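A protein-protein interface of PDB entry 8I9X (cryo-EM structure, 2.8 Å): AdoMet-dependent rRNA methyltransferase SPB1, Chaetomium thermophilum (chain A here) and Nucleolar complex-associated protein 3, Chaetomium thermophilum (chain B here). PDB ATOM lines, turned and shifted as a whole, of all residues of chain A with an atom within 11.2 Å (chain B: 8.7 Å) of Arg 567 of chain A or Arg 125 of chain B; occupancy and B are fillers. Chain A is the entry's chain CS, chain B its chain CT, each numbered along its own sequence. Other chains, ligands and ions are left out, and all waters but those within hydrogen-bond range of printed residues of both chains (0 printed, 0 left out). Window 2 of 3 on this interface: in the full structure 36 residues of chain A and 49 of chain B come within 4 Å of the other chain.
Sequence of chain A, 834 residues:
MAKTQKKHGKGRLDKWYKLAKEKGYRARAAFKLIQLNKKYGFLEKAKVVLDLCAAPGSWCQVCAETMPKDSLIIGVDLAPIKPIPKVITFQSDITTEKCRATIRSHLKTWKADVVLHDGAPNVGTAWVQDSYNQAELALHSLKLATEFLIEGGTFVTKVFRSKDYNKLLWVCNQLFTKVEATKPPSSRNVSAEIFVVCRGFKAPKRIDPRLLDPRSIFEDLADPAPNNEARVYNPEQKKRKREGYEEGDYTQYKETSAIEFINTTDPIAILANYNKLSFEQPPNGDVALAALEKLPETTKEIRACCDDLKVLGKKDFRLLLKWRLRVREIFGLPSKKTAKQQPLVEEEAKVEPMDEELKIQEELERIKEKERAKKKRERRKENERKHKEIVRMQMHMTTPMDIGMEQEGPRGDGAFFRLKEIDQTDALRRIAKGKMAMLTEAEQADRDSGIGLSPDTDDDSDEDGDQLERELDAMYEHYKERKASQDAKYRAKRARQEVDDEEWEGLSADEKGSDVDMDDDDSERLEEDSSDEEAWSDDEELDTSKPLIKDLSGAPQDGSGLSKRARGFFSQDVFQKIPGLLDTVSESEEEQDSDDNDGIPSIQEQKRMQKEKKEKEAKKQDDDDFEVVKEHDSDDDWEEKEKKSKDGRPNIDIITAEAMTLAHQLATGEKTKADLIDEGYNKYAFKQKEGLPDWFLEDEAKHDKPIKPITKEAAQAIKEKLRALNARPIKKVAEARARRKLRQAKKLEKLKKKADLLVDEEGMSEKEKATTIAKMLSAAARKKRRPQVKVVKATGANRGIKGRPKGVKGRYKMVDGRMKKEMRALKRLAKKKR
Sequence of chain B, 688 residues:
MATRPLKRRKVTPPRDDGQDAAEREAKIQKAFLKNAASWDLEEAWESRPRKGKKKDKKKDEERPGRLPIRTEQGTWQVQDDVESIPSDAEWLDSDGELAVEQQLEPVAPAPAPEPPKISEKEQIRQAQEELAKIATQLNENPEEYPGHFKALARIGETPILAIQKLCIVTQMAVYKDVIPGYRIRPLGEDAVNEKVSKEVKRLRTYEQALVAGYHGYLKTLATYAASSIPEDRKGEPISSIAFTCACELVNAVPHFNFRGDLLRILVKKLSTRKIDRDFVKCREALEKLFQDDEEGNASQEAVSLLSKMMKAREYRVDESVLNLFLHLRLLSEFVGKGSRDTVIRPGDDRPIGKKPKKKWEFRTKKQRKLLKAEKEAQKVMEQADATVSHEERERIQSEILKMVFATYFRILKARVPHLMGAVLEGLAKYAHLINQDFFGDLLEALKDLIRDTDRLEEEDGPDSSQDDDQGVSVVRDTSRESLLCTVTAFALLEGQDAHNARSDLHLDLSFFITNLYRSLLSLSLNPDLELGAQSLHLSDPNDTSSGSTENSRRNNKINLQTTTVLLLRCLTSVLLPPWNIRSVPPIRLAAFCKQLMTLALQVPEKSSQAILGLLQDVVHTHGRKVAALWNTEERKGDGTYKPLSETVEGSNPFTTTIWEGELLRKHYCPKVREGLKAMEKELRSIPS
Printed residues of chain A that touch a printed residue of chain B: Ser 563, Ala 566, Arg 567 and Phe 570. Printed residues of chain B that touch a printed residue of chain A: Arg 125, Gln 128, Glu 129 and Leu 131. Among the printed residues, 6 pairs touch across the chains.
The side-chain hydroxyl of Ser 563 of chain A sits at hydrogen-bond distance from the side-chain carboxylate of Glu 129 of chain B, at 2.7 Å. The guanidinium group (NH2) of Arg 125 of chain B lies close to the backbone NH (N) of Ser 563 of chain A (3.0 Å). The guanidinium group (NH2) of Arg 567 of chain A lies close to the guanidinium group (NH1) of Arg 125 of chain B.
The side-chain hydroxyl of Ser 563 of chain A is in hydrogen-bond range of the backbone NH of Ala 566 of chain A, 3.1 Å away. The backbone carbonyl oxygen (O) of Arg 567 of chain A is in hydrogen-bond range of the side-chain hydroxyl (OG) of Ser 571 of chain A.
Arg 567 of chain A touches just one residue of chain B: Arg 125. Printed residues of chain B within 4 Å of Phe 570 of chain A: Gln 128 (3.4 Å) and Leu 131 (3.97 Å). Leu 581 of chain A touches none of the printed residues of chain B. No residue of chain A comes within 4 Å of Ile 124 of chain B. Printed residues of chain A within 4 Å of Arg 125 of chain B: Ser 563 (3.0 Å) and Arg 567 (3.0 Å). Gln 128 of chain B touches just one residue of chain A: Phe 570. Printed residues of chain A within 4 Å of Leu 131 of chain B: Phe 570. Ala 162 of chain B touches none of the printed residues of chain A. The nearest residue of chain B that does not touch Arg 567 of chain A is Glu 129 of chain B (5.8 Å).
Among the printed residues, pairs that only touch across the chains: Ala 566 of chain A with Glu 129 of chain B (3.4 Å), Phe 570 of chain A with Gln 128 of chain B (3.4 Å) and Phe 570 of chain A with Leu 131 of chain B (3.97 Å).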
ATOM      1  N   ASP A 551      33.259 -34.155 -15.679  1.00  0.00           N
ATOM      2  CA  ASP A 551      32.091 -34.472 -16.489  1.00  0.00           C
ATOM      3  C   ASP A 551      32.514 -34.550 -17.951  1.00  0.00           C
ATOM      4  O   ASP A 551      32.914 -33.541 -18.545  1.00  0.00           O
ATOM      5  CB  ASP A 551      30.996 -33.426 -16.295  1.00  0.00           C
ATOM      6  CG  ASP A 551      29.910 -33.517 -17.349  1.00  0.00           C
ATOM      7  OD1 ASP A 551      29.156 -34.514 -17.343  1.00  0.00           O
ATOM      8  OD2 ASP A 551      29.810 -32.594 -18.184  1.00  0.00           O
ATOM      9  N   SER A 563      30.089 -20.486 -22.039  1.00  0.00           N
ATOM     10  CA  SER A 563      30.412 -21.445 -20.991  1.00  0.00           C
ATOM     11  C   SER A 563      29.471 -22.638 -21.049  1.00  0.00           C
ATOM     12  O   SER A 563      28.426 -22.576 -21.694  1.00  0.00           O
ATOM     13  CB  SER A 563      30.338 -20.786 -19.615  1.00  0.00           C
ATOM     14  OG  SER A 563      29.006 -20.430 -19.296  1.00  0.00           O
ATOM     15  N   LYS A 564      29.845 -23.727 -20.375  1.00  0.00           N
ATOM     16  CA  LYS A 564      29.000 -24.916 -20.371  1.00  0.00           C
ATOM     17  C   LYS A 564      27.650 -24.630 -19.722  1.00  0.00           C
ATOM     18  O   LYS A 564      26.607 -25.044 -20.238  1.00  0.00           O
ATOM     19  CB  LYS A 564      29.719 -26.075 -19.671  1.00  0.00           C
ATOM     20  CG  LYS A 564      30.010 -25.863 -18.193  1.00  0.00           C
ATOM     21  CD  LYS A 564      30.774 -27.038 -17.605  1.00  0.00           C
ATOM     22  CE  LYS A 564      31.040 -26.837 -16.122  1.00  0.00           C
ATOM     23  NZ  LYS A 564      31.984 -25.714 -15.872  1.00  0.00           N
ATOM     24  N   ARG A 565      27.649 -23.893 -18.610  1.00  0.00           N
ATOM     25  CA  ARG A 565      26.399 -23.555 -17.938  1.00  0.00           C
ATOM     26  C   ARG A 565      25.519 -22.678 -18.820  1.00  0.00           C
ATOM     27  O   ARG A 565      24.316 -22.926 -18.965  1.00  0.00           O
ATOM     28  CB  ARG A 565      26.703 -22.861 -16.611  1.00  0.00           C
ATOM     29  CG  ARG A 565      25.482 -22.514 -15.784  1.00  0.00           C
ATOM     30  CD  ARG A 565      25.898 -21.902 -14.458  1.00  0.00           C
ATOM     31  NE  ARG A 565      26.564 -22.876 -13.602  1.00  0.00           N
ATOM     32  CZ  ARG A 565      27.177 -22.579 -12.465  1.00  0.00           C
ATOM     33  NH1 ARG A 565      27.236 -21.335 -12.017  1.00  0.00           N
ATOM     34  NH2 ARG A 565      27.746 -23.553 -11.760  1.00  0.00           N
ATOM     35  N   ALA A 566      26.109 -21.647 -19.427  1.00  0.00           N
ATOM     36  CA  ALA A 566      25.333 -20.744 -20.270  1.00  0.00           C
ATOM     37  C   ALA A 566      24.764 -21.469 -21.484  1.00  0.00           C
ATOM     38  O   ALA A 566      23.596 -21.274 -21.841  1.00  0.00           O
ATOM     39  CB  ALA A 566      26.196 -19.562 -20.706  1.00  0.00           C
ATOM     40  N   ARG A 567      25.571 -22.312 -22.131  1.00  0.00           N
ATOM     41  CA  ARG A 567      25.140 -23.032 -23.323  1.00  0.00           C
ATOM     42  C   ARG A 567      24.252 -24.225 -23.000  1.00  0.00           C
ATOM     43  O   ARG A 567      23.638 -24.799 -23.910  1.00  0.00           O
ATOM     44  CB  ARG A 567      26.355 -23.473 -24.143  1.00  0.00           C
ATOM     45  CG  ARG A 567      26.868 -22.424 -25.128  1.00  0.00           C
ATOM     46  CD  ARG A 567      27.620 -21.299 -24.435  1.00  0.00           C
ATOM     47  NE  ARG A 567      28.217 -20.368 -25.385  1.00  0.00           N
ATOM     48  CZ  ARG A 567      29.426 -20.508 -25.913  1.00  0.00           C
ATOM     49  NH1 ARG A 567      30.198 -21.538 -25.607  1.00  0.00           N
ATOM     50  NH2 ARG A 567      29.871 -19.593 -26.769  1.00  0.00           N
ATOM     51  N   GLY A 568      24.167 -24.621 -21.733  1.00  0.00           N
ATOM     52  CA  GLY A 568      23.214 -25.641 -21.349  1.00  0.00           C
ATOM     53  C   GLY A 568      21.918 -25.045 -20.844  1.00  0.00           C
ATOM     54  O   GLY A 568      20.887 -25.724 -20.808  1.00  0.00           O
ATOM     55  N   PHE A 569      21.956 -23.771 -20.450  1.00  0.00           N
ATOM     56  CA  PHE A 569      20.742 -23.119 -19.978  1.00  0.00           C
ATOM     57  C   PHE A 569      20.010 -22.411 -21.111  1.00  0.00           C
ATOM     58  O   PHE A 569      18.815 -22.637 -21.322  1.00  0.00           O
ATOM     59  CB  PHE A 569      21.067 -22.130 -18.860  1.00  0.00           C
ATOM     60  CG  PHE A 569      19.860 -21.432 -18.306  1.00  0.00           C
ATOM     61  CD1 PHE A 569      18.995 -22.094 -17.451  1.00  0.00           C
ATOM     62  CD2 PHE A 569      19.582 -20.122 -18.650  1.00  0.00           C
ATOM     63  CE1 PHE A 569      17.879 -21.457 -16.943  1.00  0.00           C
ATOM     64  CE2 PHE A 569      18.468 -19.480 -18.146  1.00  0.00           C
ATOM     65  CZ  PHE A 569      17.615 -20.150 -17.292  1.00  0.00           C
ATOM     66  N   PHE A 570      20.704 -21.546 -21.847  1.00  0.00           N
ATOM     67  CA  PHE A 570      20.085 -20.795 -22.930  1.00  0.00           C
ATOM     68  C   PHE A 570      19.720 -21.661 -24.128  1.00  0.00           C
ATOM     69  O   PHE A 570      19.204 -21.133 -25.117  1.00  0.00           O
ATOM     70  CB  PHE A 570      21.005 -19.656 -23.377  1.00  0.00           C
ATOM     71  CG  PHE A 570      21.004 -18.478 -22.448  1.00  0.00           C
ATOM     72  CD1 PHE A 570      20.604 -17.232 -22.896  1.00  0.00           C
ATOM     73  CD2 PHE A 570      21.404 -18.615 -21.130  1.00  0.00           C
ATOM     74  CE1 PHE A 570      20.601 -16.144 -22.046  1.00  0.00           C
ATOM     75  CE2 PHE A 570      21.401 -17.531 -20.276  1.00  0.00           C
ATOM     76  CZ  PHE A 570      21.000 -16.294 -20.734  1.00  0.00           C
ATOM     77  N   SER A 571      19.973 -22.967 -24.068  1.00  0.00           N
ATOM     78  CA  SER A 571      19.635 -23.880 -25.151  1.00  0.00           C
ATOM     79  C   SER A 571      18.428 -24.741 -24.795  1.00  0.00           C
ATOM     80  O   SER A 571      18.322 -25.886 -25.237  1.00  0.00           O
ATOM     81  CB  SER A 571      20.831 -24.760 -25.513  1.00  0.00           C
ATOM     82  OG  SER A 571      21.109 -25.690 -24.482  1.00  0.00           O
ATOM     83  N   GLN A 572      17.513 -24.203 -23.996  1.00  0.00           N
ATOM     84  CA  GLN A 572      16.323 -24.938 -23.608  1.00  0.00           C
ATOM     85  C   GLN A 572      15.234 -24.823 -24.671  1.00  0.00           C
ATOM     86  O   GLN A 572      15.364 -24.108 -25.672  1.00  0.00           O
ATOM     87  CB  GLN A 572      15.801 -24.456 -22.255  1.00  0.00           C
ATOM     88  CG  GLN A 572      16.660 -24.881 -21.080  1.00  0.00           C
ATOM     89  CD  GLN A 572      16.113 -24.398 -19.752  1.00  0.00           C
ATOM     90  OE1 GLN A 572      15.119 -23.675 -19.703  1.00  0.00           O
ATOM     91  NE2 GLN A 572      16.760 -24.802 -18.664  1.00  0.00           N
ATOM     92  N   ASP A 573      14.139 -25.547 -24.428  1.00  0.00           N
ATOM     93  CA  ASP A 573      13.099 -25.694 -25.437  1.00  0.00           C
ATOM     94  C   ASP A 573      12.464 -24.358 -25.793  1.00  0.00           C
ATOM     95  O   ASP A 573      12.263 -24.063 -26.972  1.00  0.00           O
ATOM     96  CB  ASP A 573      12.036 -26.679 -24.952  1.00  0.00           C
ATOM     97  CG  ASP A 573      12.568 -28.093 -24.827  1.00  0.00           C
ATOM     98  OD1 ASP A 573      13.257 -28.385 -23.826  1.00  0.00           O
ATOM     99  OD2 ASP A 573      12.302 -28.913 -25.731  1.00  0.00           O
ATOM    100  N   PHE A 575      13.652 -21.246 -25.498  1.00  0.00           N
ATOM    101  CA  PHE A 575      14.588 -20.407 -26.235  1.00  0.00           C
ATOM    102  C   PHE A 575      14.781 -20.894 -27.663  1.00  0.00           C
ATOM    103  O   PHE A 575      14.893 -20.074 -28.580  1.00  0.00           O
ATOM    104  CB  PHE A 575      15.942 -20.346 -25.525  1.00  0.00           C
ATOM    105  CG  PHE A 575      15.858 -19.975 -24.072  1.00  0.00           C
ATOM    106  CD1 PHE A 575      16.173 -18.692 -23.658  1.00  0.00           C
ATOM    107  CD2 PHE A 575      15.506 -20.912 -23.116  1.00  0.00           C
ATOM    108  CE1 PHE A 575      16.110 -18.342 -22.325  1.00  0.00           C
ATOM    109  CE2 PHE A 575      15.438 -20.568 -21.780  1.00  0.00           C
ATOM    110  CZ  PHE A 575      15.742 -19.281 -21.384  1.00  0.00           C
ATOM    111  N   GLN A 576      14.825 -22.210 -27.874  1.00  0.00           N
ATOM    112  CA  GLN A 576      14.903 -22.721 -29.239  1.00  0.00           C
ATOM    113  C   GLN A 576      13.606 -22.454 -29.996  1.00  0.00           C
ATOM    114  O   GLN A 576      13.615 -22.255 -31.216  1.00  0.00           O
ATOM    115  CB  GLN A 576      15.228 -24.214 -29.222  1.00  0.00           C
ATOM    116  CG  GLN A 576      16.587 -24.535 -28.623  1.00  0.00           C
ATOM    117  CD  GLN A 576      17.668 -23.584 -29.098  1.00  0.00           C
ATOM    118  OE1 GLN A 576      18.056 -23.600 -30.266  1.00  0.00           O
ATOM    119  NE2 GLN A 576      18.148 -22.737 -28.196  1.00  0.00           N
ATOM    120  N   LEU A 581      16.519 -14.904 -30.878  1.00  0.00           N
ATOM    121  CA  LEU A 581      16.841 -14.641 -29.479  1.00  0.00           C
ATOM    122  C   LEU A 581      17.366 -13.221 -29.275  1.00  0.00           C
ATOM    123  O   LEU A 581      17.831 -12.579 -30.217  1.00  0.00           O
ATOM    124  CB  LEU A 581      17.858 -15.669 -28.972  1.00  0.00           C
ATOM    125  CG  LEU A 581      19.236 -15.773 -29.638  1.00  0.00           C
ATOM    126  CD1 LEU A 581      20.242 -14.768 -29.089  1.00  0.00           C
ATOM    127  CD2 LEU A 581      19.771 -17.186 -29.505  1.00  0.00           C
ATOM    128  N   GLU B 122      29.957  -9.902 -26.257  1.00  0.00           N
ATOM    129  CA  GLU B 122      29.732  -8.491 -25.978  1.00  0.00           C
ATOM    130  C   GLU B 122      29.060  -8.299 -24.627  1.00  0.00           C
ATOM    131  O   GLU B 122      29.054  -9.196 -23.773  1.00  0.00           O
ATOM    132  CB  GLU B 122      28.863  -7.851 -27.064  1.00  0.00           C
ATOM    133  CG  GLU B 122      29.513  -7.752 -28.428  1.00  0.00           C
ATOM    134  CD  GLU B 122      29.385  -9.033 -29.226  1.00  0.00           C
ATOM    135  OE1 GLU B 122      28.741  -9.981 -28.730  1.00  0.00           O
ATOM    136  OE2 GLU B 122      29.922  -9.090 -30.352  1.00  0.00           O
ATOM    137  N   GLN B 123      28.484  -7.112 -24.452  1.00  0.00           N
ATOM    138  CA  GLN B 123      27.585  -6.844 -23.343  1.00  0.00           C
ATOM    139  C   GLN B 123      26.468  -7.867 -23.277  1.00  0.00           C
ATOM    140  O   GLN B 123      26.064  -8.264 -22.179  1.00  0.00           O
ATOM    141  CB  GLN B 123      26.984  -5.440 -23.470  1.00  0.00           C
ATOM    142  CG  GLN B 123      27.992  -4.301 -23.542  1.00  0.00           C
ATOM    143  CD  GLN B 123      28.635  -4.168 -24.912  1.00  0.00           C
ATOM    144  OE1 GLN B 123      29.850  -4.297 -25.058  1.00  0.00           O
ATOM    145  NE2 GLN B 123      27.816  -3.914 -25.927  1.00  0.00           N
ATOM    146  N   ILE B 124      25.980  -8.310 -24.430  1.00  0.00           N
ATOM    147  CA  ILE B 124      24.953  -9.340 -24.495  1.00  0.00           C
ATOM    148  C   ILE B 124      25.437 -10.641 -23.874  1.00  0.00           C
ATOM    149  O   ILE B 124      24.726 -11.252 -23.075  1.00  0.00           O
ATOM    150  CB  ILE B 124      24.504  -9.546 -25.957  1.00  0.00           C
ATOM    151  CG1 ILE B 124      23.868  -8.271 -26.524  1.00  0.00           C
ATOM    152  CG2 ILE B 124      23.527 -10.697 -26.056  1.00  0.00           C
ATOM    153  CD1 ILE B 124      24.849  -7.310 -27.175  1.00  0.00           C
ATOM    154  N   ARG B 125      26.651 -11.085 -24.215  1.00  0.00           N
ATOM    155  CA  ARG B 125      27.174 -12.309 -23.616  1.00  0.00           C
ATOM    156  C   ARG B 125      27.429 -12.142 -22.125  1.00  0.00           C
ATOM    157  O   ARG B 125      27.202 -13.080 -21.351  1.00  0.00           O
ATOM    158  CB  ARG B 125      28.456 -12.752 -24.321  1.00  0.00           C
ATOM    159  CG  ARG B 125      28.996 -14.068 -23.780  1.00  0.00           C
ATOM    160  CD  ARG B 125      30.206 -14.567 -24.545  1.00  0.00           C
ATOM    161  NE  ARG B 125      30.747 -15.778 -23.936  1.00  0.00           N
ATOM    162  CZ  ARG B 125      30.319 -17.004 -24.202  1.00  0.00           C
ATOM    163  NH1 ARG B 125      29.334 -17.222 -25.057  1.00  0.00           N
ATOM    164  NH2 ARG B 125      30.888 -18.038 -23.589  1.00  0.00           N
ATOM    165  N   GLN B 126      27.904 -10.969 -21.703  1.00  0.00           N
ATOM    166  CA  GLN B 126      28.069 -10.723 -20.275  1.00  0.00           C
ATOM    167  C   GLN B 126      26.733 -10.850 -19.552  1.00  0.00           C
ATOM    168  O   GLN B 126      26.640 -11.465 -18.481  1.00  0.00           O
ATOM    169  CB  GLN B 126      28.678  -9.338 -20.051  1.00  0.00           C
ATOM    170  CG  GLN B 126      28.984  -9.014 -18.599  1.00  0.00           C
ATOM    171  CD  GLN B 126      30.106  -9.865 -18.036  1.00  0.00           C
ATOM    172  OE1 GLN B 126      31.106 -10.116 -18.706  1.00  0.00           O
ATOM    173  NE2 GLN B 126      29.944 -10.313 -16.796  1.00  0.00           N
ATOM    174  N   ALA B 127      25.679 -10.285 -20.140  1.00  0.00           N
ATOM    175  CA  ALA B 127      24.352 -10.382 -19.546  1.00  0.00           C
ATOM    176  C   ALA B 127      23.866 -11.824 -19.515  1.00  0.00           C
ATOM    177  O   ALA B 127      23.249 -12.254 -18.537  1.00  0.00           O
ATOM    178  CB  ALA B 127      23.368  -9.500 -20.310  1.00  0.00           C
ATOM    179  N   GLN B 128      24.121 -12.584 -20.585  1.00  0.00           N
ATOM    180  CA  GLN B 128      23.724 -13.990 -20.587  1.00  0.00           C
ATOM    181  C   GLN B 128      24.422 -14.758 -19.478  1.00  0.00           C
ATOM    182  O   GLN B 128      23.803 -15.588 -18.805  1.00  0.00           O
ATOM    183  CB  GLN B 128      24.012 -14.650 -21.937  1.00  0.00           C
ATOM    184  CG  GLN B 128      23.393 -13.981 -23.145  1.00  0.00           C
ATOM    185  CD  GLN B 128      23.952 -14.523 -24.445  1.00  0.00           C
ATOM    186  OE1 GLN B 128      24.681 -15.514 -24.452  1.00  0.00           O
ATOM    187  NE2 GLN B 128      23.602 -13.886 -25.554  1.00  0.00           N
ATOM    188  N   GLU B 129      25.714 -14.501 -19.277  1.00  0.00           N
ATOM    189  CA  GLU B 129      26.434 -15.162 -18.194  1.00  0.00           C
ATOM    190  C   GLU B 129      25.843 -14.784 -16.841  1.00  0.00           C
ATOM    191  O   GLU B 129      25.675 -15.640 -15.962  1.00  0.00           O
ATOM    192  CB  GLU B 129      27.920 -14.807 -18.256  1.00  0.00           C
ATOM    193  CG  GLU B 129      28.703 -15.579 -19.312  1.00  0.00           C
ATOM    194  CD  GLU B 129      28.768 -17.072 -19.038  1.00  0.00           C
ATOM    195  OE1 GLU B 129      28.531 -17.487 -17.882  1.00  0.00           O
ATOM    196  OE2 GLU B 129      29.056 -17.834 -19.983  1.00  0.00           O
ATOM    197  N   GLU B 130      25.513 -13.502 -16.661  1.00  0.00           N
ATOM    198  CA  GLU B 130      24.902 -13.072 -15.407  1.00  0.00           C
ATOM    199  C   GLU B 130      23.579 -13.791 -15.160  1.00  0.00           C
ATOM    200  O   GLU B 130      23.359 -14.343 -14.074  1.00  0.00           O
ATOM    201  CB  GLU B 130      24.696 -11.558 -15.415  1.00  0.00           C
ATOM    202  CG  GLU B 130      24.101 -11.002 -14.129  1.00  0.00           C
ATOM    203  CD  GLU B 130      25.021 -11.170 -12.934  1.00  0.00           C
ATOM    204  OE1 GLU B 130      26.252 -11.247 -13.131  1.00  0.00           O
ATOM    205  OE2 GLU B 130      24.513 -11.224 -11.794  1.00  0.00           O
ATOM    206  N   LEU B 131      22.695 -13.807 -16.160  1.00  0.00           N
ATOM    207  CA  LEU B 131      21.402 -14.470 -16.004  1.00  0.00           C
ATOM    208  C   LEU B 131      21.572 -15.961 -15.754  1.00  0.00           C
ATOM    209  O   LEU B 131      20.824 -16.557 -14.970  1.00  0.00           O
ATOM    210  CB  LEU B 131      20.519 -14.236 -17.231  1.00  0.00           C
ATOM    211  CG  LEU B 131      20.383 -12.833 -17.817  1.00  0.00           C
ATOM    212  CD1 LEU B 131      19.699 -12.883 -19.171  1.00  0.00           C
ATOM    213  CD2 LEU B 131      19.605 -11.952 -16.865  1.00  0.00           C
ATOM    214  N   ALA B 132      22.529 -16.591 -16.435  1.00  0.00           N
ATOM    215  CA  ALA B 132      22.769 -18.011 -16.215  1.00  0.00           C
ATOM    216  C   ALA B 132      23.190 -18.273 -14.778  1.00  0.00           C
ATOM    217  O   ALA B 132      22.685 -19.204 -14.139  1.00  0.00           O
ATOM    218  CB  ALA B 132      23.827 -18.524 -17.191  1.00  0.00           C
ATOM    219  N   LYS B 133      24.102 -17.453 -14.250  1.00  0.00           N
ATOM    220  CA  LYS B 133      24.498 -17.592 -12.853  1.00  0.00           C
ATOM    221  C   LYS B 133      23.294 -17.441 -11.933  1.00  0.00           C
ATOM    222  O   LYS B 133      23.081 -18.252 -11.022  1.00  0.00           O
ATOM    223  CB  LYS B 133      25.573 -16.561 -12.506  1.00  0.00           C
ATOM    224  CG  LYS B 133      26.900 -16.761 -13.220  1.00  0.00           C
ATOM    225  CD  LYS B 133      27.864 -15.629 -12.899  1.00  0.00           C
ATOM    226  CE  LYS B 133      29.147 -15.743 -13.705  1.00  0.00           C
ATOM    227  NZ  LYS B 133      30.066 -14.600 -13.446  1.00  0.00           N
ATOM    228  N   ILE B 160      19.042  -1.930 -24.081  1.00  0.00           N
ATOM    229  CA  ILE B 160      19.188  -2.562 -25.389  1.00  0.00           C
ATOM    230  C   ILE B 160      18.222  -3.735 -25.520  1.00  0.00           C
ATOM    231  O   ILE B 160      18.029  -4.531 -24.584  1.00  0.00           O
ATOM    232  CB  ILE B 160      20.645  -2.971 -25.650  1.00  0.00           C
ATOM    233  CG1 ILE B 160      21.148  -4.000 -24.647  1.00  0.00           C
ATOM    234  CG2 ILE B 160      21.547  -1.745 -25.638  1.00  0.00           C
ATOM    235  CD1 ILE B 160      22.491  -4.561 -25.055  1.00  0.00           C
ATOM    236  N   ALA B 162      17.886  -6.572 -27.194  1.00  0.00           N
ATOM    237  CA  ALA B 162      18.230  -7.982 -27.081  1.00  0.00           C
ATOM    238  C   ALA B 162      18.284  -8.422 -25.627  1.00  0.00           C
ATOM    239  O   ALA B 162      17.695  -9.450 -25.264  1.00  0.00           O
ATOM    240  CB  ALA B 162      19.566  -8.257 -27.772  1.00  0.00           C
ATOM    241  N   ILE B 163      18.952  -7.650 -24.779  1.00  0.00           N
ATOM    242  CA  ILE B 163      19.019  -8.016 -23.373  1.00  0.00           C
ATOM    243  C   ILE B 163      17.666  -7.845 -22.696  1.00  0.00           C
ATOM    244  O   ILE B 163      17.336  -8.605 -21.786  1.00  0.00           O
ATOM    245  CB  ILE B 163      20.128  -7.236 -22.642  1.00  0.00           C
ATOM    246  CG1 ILE B 163      21.493  -7.577 -23.237  1.00  0.00           C
ATOM    247  CG2 ILE B 163      20.163  -7.614 -21.172  1.00  0.00           C
ATOM    248  CD1 ILE B 163      22.645  -6.882 -22.543  1.00  0.00           C
ATOM    249  N   LEU B 166      15.920 -11.069 -23.532  1.00  0.00           N
ATOM    250  CA  LEU B 166      16.531 -12.175 -22.808  1.00  0.00           C
ATOM    251  C   LEU B 166      16.154 -12.156 -21.336  1.00  0.00           C
ATOM    252  O   LEU B 166      15.825 -13.204 -20.770  1.00  0.00           O
ATOM    253  CB  LEU B 166      18.050 -12.141 -22.972  1.00  0.00           C
ATOM    254  CG  LEU B 166      18.577 -12.407 -24.382  1.00  0.00           C
ATOM    255  CD1 LEU B 166      20.018 -11.944 -24.514  1.00  0.00           C
ATOM    256  CD2 LEU B 166      18.449 -13.882 -24.733  1.00  0.00           C
